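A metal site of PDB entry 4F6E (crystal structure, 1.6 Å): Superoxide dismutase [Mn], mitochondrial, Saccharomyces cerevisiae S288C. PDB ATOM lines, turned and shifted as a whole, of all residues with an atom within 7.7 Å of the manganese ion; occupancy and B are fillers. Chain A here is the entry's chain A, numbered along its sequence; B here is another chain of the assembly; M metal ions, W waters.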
ATOM      1  N   HIS A  26       2.902   0.023 -24.841  1.00  0.00           N
ATOM      2  CA  HIS A  26       3.883  -0.866 -24.249  1.00  0.00           C
ATOM      3  C   HIS A  26       3.236  -2.207 -23.885  1.00  0.00           C
ATOM      4  O   HIS A  26       3.833  -3.269 -24.077  1.00  0.00           O
ATOM      5  CB  HIS A  26       4.480  -0.173 -23.019  1.00  0.00           C
ATOM      6  CG  HIS A  26       5.821  -0.700 -22.632  1.00  0.00           C
ATOM      7  ND1 HIS A  26       6.552  -0.172 -21.588  1.00  0.00           N
ATOM      8  CD2 HIS A  26       6.575  -1.684 -23.161  1.00  0.00           C
ATOM      9  CE1 HIS A  26       7.684  -0.828 -21.468  1.00  0.00           C
ATOM     10  NE2 HIS A  26       7.726  -1.753 -22.412  1.00  0.00           N
ATOM     11  N   TYR A  27       1.999  -2.150 -23.371  1.00  0.00           N
ATOM     12  CA  TYR A  27       1.249  -3.327 -22.961  1.00  0.00           C
ATOM     13  C   TYR A  27       0.534  -4.007 -24.135  1.00  0.00           C
ATOM     14  O   TYR A  27       0.736  -5.205 -24.399  1.00  0.00           O
ATOM     15  CB  TYR A  27       0.238  -2.902 -21.890  1.00  0.00           C
ATOM     16  CG  TYR A  27      -0.658  -4.002 -21.337  1.00  0.00           C
ATOM     17  CD1 TYR A  27      -0.194  -4.896 -20.382  1.00  0.00           C
ATOM     18  CD2 TYR A  27      -1.987  -4.094 -21.733  1.00  0.00           C
ATOM     19  CE1 TYR A  27      -1.032  -5.873 -19.849  1.00  0.00           C
ATOM     20  CE2 TYR A  27      -2.816  -5.068 -21.201  1.00  0.00           C
ATOM     21  CZ  TYR A  27      -2.334  -5.956 -20.270  1.00  0.00           C
ATOM     22  OH  TYR A  27      -3.163  -6.929 -19.737  1.00  0.00           O
ATOM     23  N   HIS A  30       3.678  -4.028 -27.577  1.00  0.00           N
ATOM     24  CA  HIS A  30       4.974  -4.635 -27.321  1.00  0.00           C
ATOM     25  C   HIS A  30       4.871  -5.926 -26.502  1.00  0.00           C
ATOM     26  O   HIS A  30       5.349  -6.979 -26.917  1.00  0.00           O
ATOM     27  CB  HIS A  30       5.947  -3.620 -26.680  1.00  0.00           C
ATOM     28  CG  HIS A  30       6.279  -2.463 -27.562  1.00  0.00           C
ATOM     29  ND1 HIS A  30       7.228  -2.545 -28.569  1.00  0.00           N
ATOM     30  CD2 HIS A  30       5.772  -1.213 -27.625  1.00  0.00           C
ATOM     31  CE1 HIS A  30       7.289  -1.383 -29.198  1.00  0.00           C
ATOM     32  NE2 HIS A  30       6.426  -0.560 -28.653  1.00  0.00           N
ATOM     33  N   HIS A  31       4.227  -5.850 -25.338  1.00  0.00           N
ATOM     34  CA  HIS A  31       4.122  -7.050 -24.516  1.00  0.00           C
ATOM     35  C   HIS A  31       3.316  -8.128 -25.244  1.00  0.00           C
ATOM     36  O   HIS A  31       3.676  -9.301 -25.182  1.00  0.00           O
ATOM     37  CB  HIS A  31       3.507  -6.725 -23.148  1.00  0.00           C
ATOM     38  CG  HIS A  31       3.779  -7.772 -22.110  1.00  0.00           C
ATOM     39  ND1 HIS A  31       3.315  -7.660 -20.820  1.00  0.00           N
ATOM     40  CD2 HIS A  31       4.467  -8.933 -22.176  1.00  0.00           C
ATOM     41  CE1 HIS A  31       3.714  -8.718 -20.125  1.00  0.00           C
ATOM     42  NE2 HIS A  31       4.414  -9.508 -20.927  1.00  0.00           N
ATOM     43  N   TYR A  34       5.489 -10.198 -27.592  1.00  0.00           N
ATOM     44  CA  TYR A  34       6.257 -11.239 -26.911  1.00  0.00           C
ATOM     45  C   TYR A  34       5.379 -12.418 -26.493  1.00  0.00           C
ATOM     46  O   TYR A  34       5.809 -13.555 -26.577  1.00  0.00           O
ATOM     47  CB  TYR A  34       6.987 -10.672 -25.686  1.00  0.00           C
ATOM     48  CG  TYR A  34       7.938  -9.558 -26.037  1.00  0.00           C
ATOM     49  CD1 TYR A  34       8.920  -9.745 -26.994  1.00  0.00           C
ATOM     50  CD2 TYR A  34       7.820  -8.315 -25.444  1.00  0.00           C
ATOM     51  CE1 TYR A  34       9.788  -8.721 -27.340  1.00  0.00           C
ATOM     52  CE2 TYR A  34       8.684  -7.278 -25.772  1.00  0.00           C
ATOM     53  CZ  TYR A  34       9.656  -7.493 -26.727  1.00  0.00           C
ATOM     54  OH  TYR A  34      10.501  -6.462 -27.053  1.00  0.00           O
ATOM     55  N   GLY A  77      10.991 -11.496 -23.167  1.00  0.00           N
ATOM     56  CA  GLY A  77      10.116 -10.342 -23.314  1.00  0.00           C
ATOM     57  C   GLY A  77       8.835 -10.526 -22.500  1.00  0.00           C
ATOM     58  O   GLY A  77       8.345  -9.589 -21.854  1.00  0.00           O
ATOM     59  N   ASN A  80      10.019 -10.428 -18.582  1.00  0.00           N
ATOM     60  CA  ASN A  80      10.528  -9.134 -18.105  1.00  0.00           C
ATOM     61  C   ASN A  80       9.424  -8.108 -17.984  1.00  0.00           C
ATOM     62  O   ASN A  80       9.405  -7.327 -17.038  1.00  0.00           O
ATOM     63  CB  ASN A  80      11.627  -8.584 -19.037  1.00  0.00           C
ATOM     64  CG  ASN A  80      12.956  -9.297 -18.875  1.00  0.00           C
ATOM     65  OD1 ASN A  80      13.273  -9.875 -17.837  1.00  0.00           O
ATOM     66  ND2 ASN A  80      13.764  -9.248 -19.940  1.00  0.00           N
ATOM     67  N   HIS A  81       8.492  -8.096 -18.940  1.00  0.00           N
ATOM     68  CA  HIS A  81       7.384  -7.155 -18.863  1.00  0.00           C
ATOM     69  C   HIS A  81       6.412  -7.491 -17.754  1.00  0.00           C
ATOM     70  O   HIS A  81       5.872  -6.592 -17.111  1.00  0.00           O
ATOM     71  CB  HIS A  81       6.686  -6.966 -20.211  1.00  0.00           C
ATOM     72  CG  HIS A  81       7.528  -6.234 -21.197  1.00  0.00           C
ATOM     73  ND1 HIS A  81       8.484  -6.871 -21.965  1.00  0.00           N
ATOM     74  CD2 HIS A  81       7.634  -4.922 -21.478  1.00  0.00           C
ATOM     75  CE1 HIS A  81       9.102  -5.982 -22.713  1.00  0.00           C
ATOM     76  NE2 HIS A  81       8.601  -4.789 -22.436  1.00  0.00           N
ATOM     77  N   PHE A  84       8.002  -6.069 -14.745  1.00  0.00           N
ATOM     78  CA  PHE A  84       7.970  -4.607 -14.835  1.00  0.00           C
ATOM     79  C   PHE A  84       6.641  -4.067 -14.349  1.00  0.00           C
ATOM     80  O   PHE A  84       6.603  -3.220 -13.459  1.00  0.00           O
ATOM     81  CB  PHE A  84       8.232  -4.204 -16.301  1.00  0.00           C
ATOM     82  CG  PHE A  84       8.453  -2.730 -16.522  1.00  0.00           C
ATOM     83  CD1 PHE A  84       9.418  -2.042 -15.812  1.00  0.00           C
ATOM     84  CD2 PHE A  84       7.714  -2.044 -17.484  1.00  0.00           C
ATOM     85  CE1 PHE A  84       9.642  -0.687 -16.027  1.00  0.00           C
ATOM     86  CE2 PHE A  84       7.942  -0.702 -17.717  1.00  0.00           C
ATOM     87  CZ  PHE A  84       8.899  -0.021 -16.996  1.00  0.00           C
ATOM     88  N   TRP A  85       5.535  -4.573 -14.886  1.00  0.00           N
ATOM     89  CA  TRP A  85       4.240  -4.023 -14.470  1.00  0.00           C
ATOM     90  C   TRP A  85       4.009  -4.226 -12.986  1.00  0.00           C
ATOM     91  O   TRP A  85       3.424  -3.373 -12.329  1.00  0.00           O
ATOM     92  CB  TRP A  85       3.054  -4.621 -15.236  1.00  0.00           C
ATOM     93  CG  TRP A  85       3.199  -4.700 -16.725  1.00  0.00           C
ATOM     94  CD1 TRP A  85       2.959  -5.805 -17.498  1.00  0.00           C
ATOM     95  CD2 TRP A  85       3.598  -3.668 -17.640  1.00  0.00           C
ATOM     96  NE1 TRP A  85       3.177  -5.534 -18.819  1.00  0.00           N
ATOM     97  CE2 TRP A  85       3.581  -4.235 -18.934  1.00  0.00           C
ATOM     98  CE3 TRP A  85       3.977  -2.330 -17.490  1.00  0.00           C
ATOM     99  CZ2 TRP A  85       3.929  -3.508 -20.070  1.00  0.00           C
ATOM    100  CZ3 TRP A  85       4.323  -1.600 -18.635  1.00  0.00           C
ATOM    101  CH2 TRP A  85       4.287  -2.197 -19.904  1.00  0.00           C
ATOM    102  N   GLY A 132      17.910  -2.901 -23.499  1.00  0.00           N
ATOM    103  CA  GLY A 132      18.095  -3.821 -22.401  1.00  0.00           C
ATOM    104  C   GLY A 132      17.371  -3.375 -21.146  1.00  0.00           C
ATOM    105  O   GLY A 132      16.426  -2.582 -21.223  1.00  0.00           O
ATOM    106  N   TRP A 133      17.850  -3.877 -20.005  1.00  0.00           N
ATOM    107  CA  TRP A 133      17.189  -3.754 -18.708  1.00  0.00           C
ATOM    108  C   TRP A 133      18.235  -3.564 -17.632  1.00  0.00           C
ATOM    109  O   TRP A 133      19.380  -3.976 -17.791  1.00  0.00           O
ATOM    110  CB  TRP A 133      16.456  -5.072 -18.358  1.00  0.00           C
ATOM    111  CG  TRP A 133      15.275  -5.345 -19.237  1.00  0.00           C
ATOM    112  CD1 TRP A 133      15.309  -5.844 -20.515  1.00  0.00           C
ATOM    113  CD2 TRP A 133      13.903  -5.070 -18.957  1.00  0.00           C
ATOM    114  NE1 TRP A 133      14.036  -5.910 -21.024  1.00  0.00           N
ATOM    115  CE2 TRP A 133      13.152  -5.450 -20.080  1.00  0.00           C
ATOM    116  CE3 TRP A 133      13.227  -4.580 -17.829  1.00  0.00           C
ATOM    117  CZ2 TRP A 133      11.750  -5.337 -20.134  1.00  0.00           C
ATOM    118  CZ3 TRP A 133      11.832  -4.456 -17.880  1.00  0.00           C
ATOM    119  CH2 TRP A 133      11.121  -4.835 -19.023  1.00  0.00           C
ATOM    120  N   ASN A 153      18.784  -6.638 -24.599  1.00  0.00           N
ATOM    121  CA  ASN A 153      17.644  -7.132 -25.356  1.00  0.00           C
ATOM    122  C   ASN A 153      16.560  -7.667 -24.443  1.00  0.00           C
ATOM    123  O   ASN A 153      16.110  -6.927 -23.577  1.00  0.00           O
ATOM    124  CB  ASN A 153      18.122  -8.122 -26.407  1.00  0.00           C
ATOM    125  CG  ASN A 153      19.183  -7.494 -27.287  1.00  0.00           C
ATOM    126  OD1 ASN A 153      19.024  -6.357 -27.709  1.00  0.00           O
ATOM    127  ND2 ASN A 153      20.294  -8.189 -27.486  1.00  0.00           N
ATOM    128  N   GLN A 154      16.158  -8.918 -24.597  1.00  0.00           N
ATOM    129  CA  GLN A 154      15.234  -9.495 -23.629  1.00  0.00           C
ATOM    130  C   GLN A 154      15.876 -10.597 -22.789  1.00  0.00           C
ATOM    131  O   GLN A 154      15.191 -11.467 -22.248  1.00  0.00           O
ATOM    132  CB  GLN A 154      13.926  -9.977 -24.286  1.00  0.00           C
ATOM    133  CG  GLN A 154      13.089  -8.856 -24.918  1.00  0.00           C
ATOM    134  CD  GLN A 154      12.649  -7.781 -23.919  1.00  0.00           C
ATOM    135  OE1 GLN A 154      12.734  -7.967 -22.702  1.00  0.00           O
ATOM    136  NE2 GLN A 154      12.176  -6.664 -24.452  1.00  0.00           N
ATOM    137  N   ASP A 168      12.923  -1.138 -17.445  1.00  0.00           N
ATOM    138  CA  ASP A 168      13.053  -1.279 -18.889  1.00  0.00           C
ATOM    139  C   ASP A 168      13.820  -0.101 -19.480  1.00  0.00           C
ATOM    140  O   ASP A 168      13.427   1.049 -19.278  1.00  0.00           O
ATOM    141  CB  ASP A 168      11.645  -1.348 -19.489  1.00  0.00           C
ATOM    142  CG  ASP A 168      11.605  -1.799 -20.919  1.00  0.00           C
ATOM    143  OD1 ASP A 168      12.656  -2.067 -21.539  1.00  0.00           O
ATOM    144  OD2 ASP A 168      10.473  -1.867 -21.418  1.00  0.00           O
ATOM    145  N   ALA A 169      14.912  -0.381 -20.192  1.00  0.00           N
ATOM    146  CA  ALA A 169      15.703   0.664 -20.852  1.00  0.00           C
ATOM    147  C   ALA A 169      15.578   0.637 -22.378  1.00  0.00           C
ATOM    148  O   ALA A 169      16.308   1.360 -23.065  1.00  0.00           O
ATOM    149  CB  ALA A 169      17.189   0.573 -20.445  1.00  0.00           C
ATOM    150  N   TRP A 170      14.676  -0.179 -22.923  1.00  0.00           N
ATOM    151  CA  TRP A 170      14.410  -0.099 -24.361  1.00  0.00           C
ATOM    152  C   TRP A 170      13.847   1.269 -24.683  1.00  0.00           C
ATOM    153  O   TRP A 170      13.116   1.860 -23.876  1.00  0.00           O
ATOM    154  CB  TRP A 170      13.391  -1.148 -24.796  1.00  0.00           C
ATOM    155  CG  TRP A 170      13.922  -2.536 -24.960  1.00  0.00           C
ATOM    156  CD1 TRP A 170      14.553  -3.303 -24.005  1.00  0.00           C
ATOM    157  CD2 TRP A 170      13.830  -3.354 -26.127  1.00  0.00           C
ATOM    158  NE1 TRP A 170      14.856  -4.539 -24.529  1.00  0.00           N
ATOM    159  CE2 TRP A 170      14.418  -4.598 -25.828  1.00  0.00           C
ATOM    160  CE3 TRP A 170      13.303  -3.149 -27.410  1.00  0.00           C
ATOM    161  CZ2 TRP A 170      14.506  -5.639 -26.763  1.00  0.00           C
ATOM    162  CZ3 TRP A 170      13.396  -4.173 -28.328  1.00  0.00           C
ATOM    163  CH2 TRP A 170      13.983  -5.407 -28.002  1.00  0.00           C
ATOM    164  N   GLU A 171      14.177   1.781 -25.868  1.00  0.00           N
ATOM    165  CA  GLU A 171      13.722   3.107 -26.243  1.00  0.00           C
ATOM    166  C   GLU A 171      12.192   3.224 -26.277  1.00  0.00           C
ATOM    167  O   GLU A 171      11.651   4.278 -25.958  1.00  0.00           O
ATOM    168  CB  GLU A 171      14.368   3.520 -27.576  1.00  0.00           C
ATOM    169  CG  GLU A 171      15.873   3.802 -27.421  1.00  0.00           C
ATOM    170  CD  GLU A 171      16.574   4.218 -28.721  1.00  0.00           C
ATOM    171  OE1 GLU A 171      16.323   3.588 -29.764  1.00  0.00           O
ATOM    172  OE2 GLU A 171      17.419   5.138 -28.650  1.00  0.00           O
ATOM    173  N   HIS A 172      11.490   2.129 -26.606  1.00  0.00           N
ATOM    174  CA  HIS A 172      10.025   2.194 -26.609  1.00  0.00           C
ATOM    175  C   HIS A 172       9.443   2.437 -25.216  1.00  0.00           C
ATOM    176  O   HIS A 172       8.268   2.754 -25.098  1.00  0.00           O
ATOM    177  CB  HIS A 172       9.364   0.956 -27.237  1.00  0.00           C
ATOM    178  CG  HIS A 172       9.582  -0.314 -26.475  1.00  0.00           C
ATOM    179  ND1 HIS A 172      10.213  -1.405 -27.040  1.00  0.00           N
ATOM    180  CD2 HIS A 172       9.212  -0.681 -25.233  1.00  0.00           C
ATOM    181  CE1 HIS A 172      10.243  -2.388 -26.162  1.00  0.00           C
ATOM    182  NE2 HIS A 172       9.650  -1.978 -25.052  1.00  0.00           N
ATOM    183  N   ALA A 173      10.252   2.261 -24.176  1.00  0.00           N
ATOM    184  CA  ALA A 173       9.760   2.484 -22.823  1.00  0.00           C
ATOM    185  C   ALA A 173       9.627   3.967 -22.472  1.00  0.00           C
ATOM    186  O   ALA A 173       8.977   4.303 -21.489  1.00  0.00           O
ATOM    187  CB  ALA A 173      10.643   1.751 -21.781  1.00  0.00           C
ATOM    188  N   TYR A 185      14.109  10.020 -17.911  1.00  0.00           N
ATOM    189  CA  TYR A 185      13.205   8.895 -17.697  1.00  0.00           C
ATOM    190  C   TYR A 185      13.674   8.065 -16.509  1.00  0.00           C
ATOM    191  O   TYR A 185      12.880   7.688 -15.645  1.00  0.00           O
ATOM    192  CB  TYR A 185      13.127   8.047 -18.957  1.00  0.00           C
ATOM    193  CG  TYR A 185      12.625   6.620 -18.794  1.00  0.00           C
ATOM    194  CD1 TYR A 185      11.295   6.353 -18.444  1.00  0.00           C
ATOM    195  CD2 TYR A 185      13.470   5.542 -19.040  1.00  0.00           C
ATOM    196  CE1 TYR A 185      10.848   5.028 -18.308  1.00  0.00           C
ATOM    197  CE2 TYR A 185      13.028   4.234 -18.909  1.00  0.00           C
ATOM    198  CZ  TYR A 185      11.716   3.978 -18.548  1.00  0.00           C
ATOM    199  OH  TYR A 185      11.274   2.665 -18.431  1.00  0.00           O
ATOM    200  N   GLU B 171      15.040   1.739 -32.343  1.00  0.00           N
ATOM    201  CA  GLU B 171      13.710   2.324 -32.192  1.00  0.00           C
ATOM    202  C   GLU B 171      13.698   3.853 -32.380  1.00  0.00           C
ATOM    203  O   GLU B 171      12.738   4.393 -32.908  1.00  0.00           O
ATOM    204  CB  GLU B 171      13.081   1.894 -30.859  1.00  0.00           C
ATOM    205  CG  GLU B 171      12.813   0.390 -30.826  1.00  0.00           C
ATOM    206  CD  GLU B 171      12.175  -0.102 -29.516  1.00  0.00           C
ATOM    207  OE1 GLU B 171      12.663   0.280 -28.441  1.00  0.00           O
ATOM    208  OE2 GLU B 171      11.199  -0.882 -29.610  1.00  0.00           O
HETATM  209 MN    MN M   1       9.598  -2.898 -23.038  1.00  0.00          MN
HETATM  210  O   HOH W   1      11.662  -4.007 -23.385  1.00  0.00           O
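Four residues have an atom within 4 Å of the manganese ion: His 26, His 81, Asp 168 and His 172. The nearest printed residue that does not touch the manganese ion is Trp 133 (4.4 Å).
The manganese ion is bound by the side-chain carboxylate of Asp 168, a ring nitrogen (NE2) of His 172, a ring nitrogen (NE2) of His 81, a ring nitrogen (NE2) of His 26 and water W1.
OD1 of Asp 168 sits at hydrogen-bond distance from N of Trp 170, 3.1 Å away. The backbone carbonyl oxygen (O) of Asp 168 sits at hydrogen-bond distance from the side-chain hydroxyl (OH) of Tyr 185, 2.8 Å away. ND1 of His 172 lies within hydrogen-bond range of OE2 of Glu 171 of chain B, 2.8 Å away. The indole nitrogen (NE1) of Trp 85 lies close to the backbone carbonyl oxygen (O) of His 81 (3.4 Å). The backbone carbonyl oxygen of Gly 77 lies within hydrogen-bond range of a ring nitrogen (ND1) of His 81, 2.7 Å away. N of His 31 lies within hydrogen-bond range of O of His 26 (2.9 Å).
Water W1 lies within hydrogen-bond range of OD1 of Asp 168 (2.9 Å), NE2 of Gln 154 (2.9 Å) and NE1 of Trp 170 (3.4 Å).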
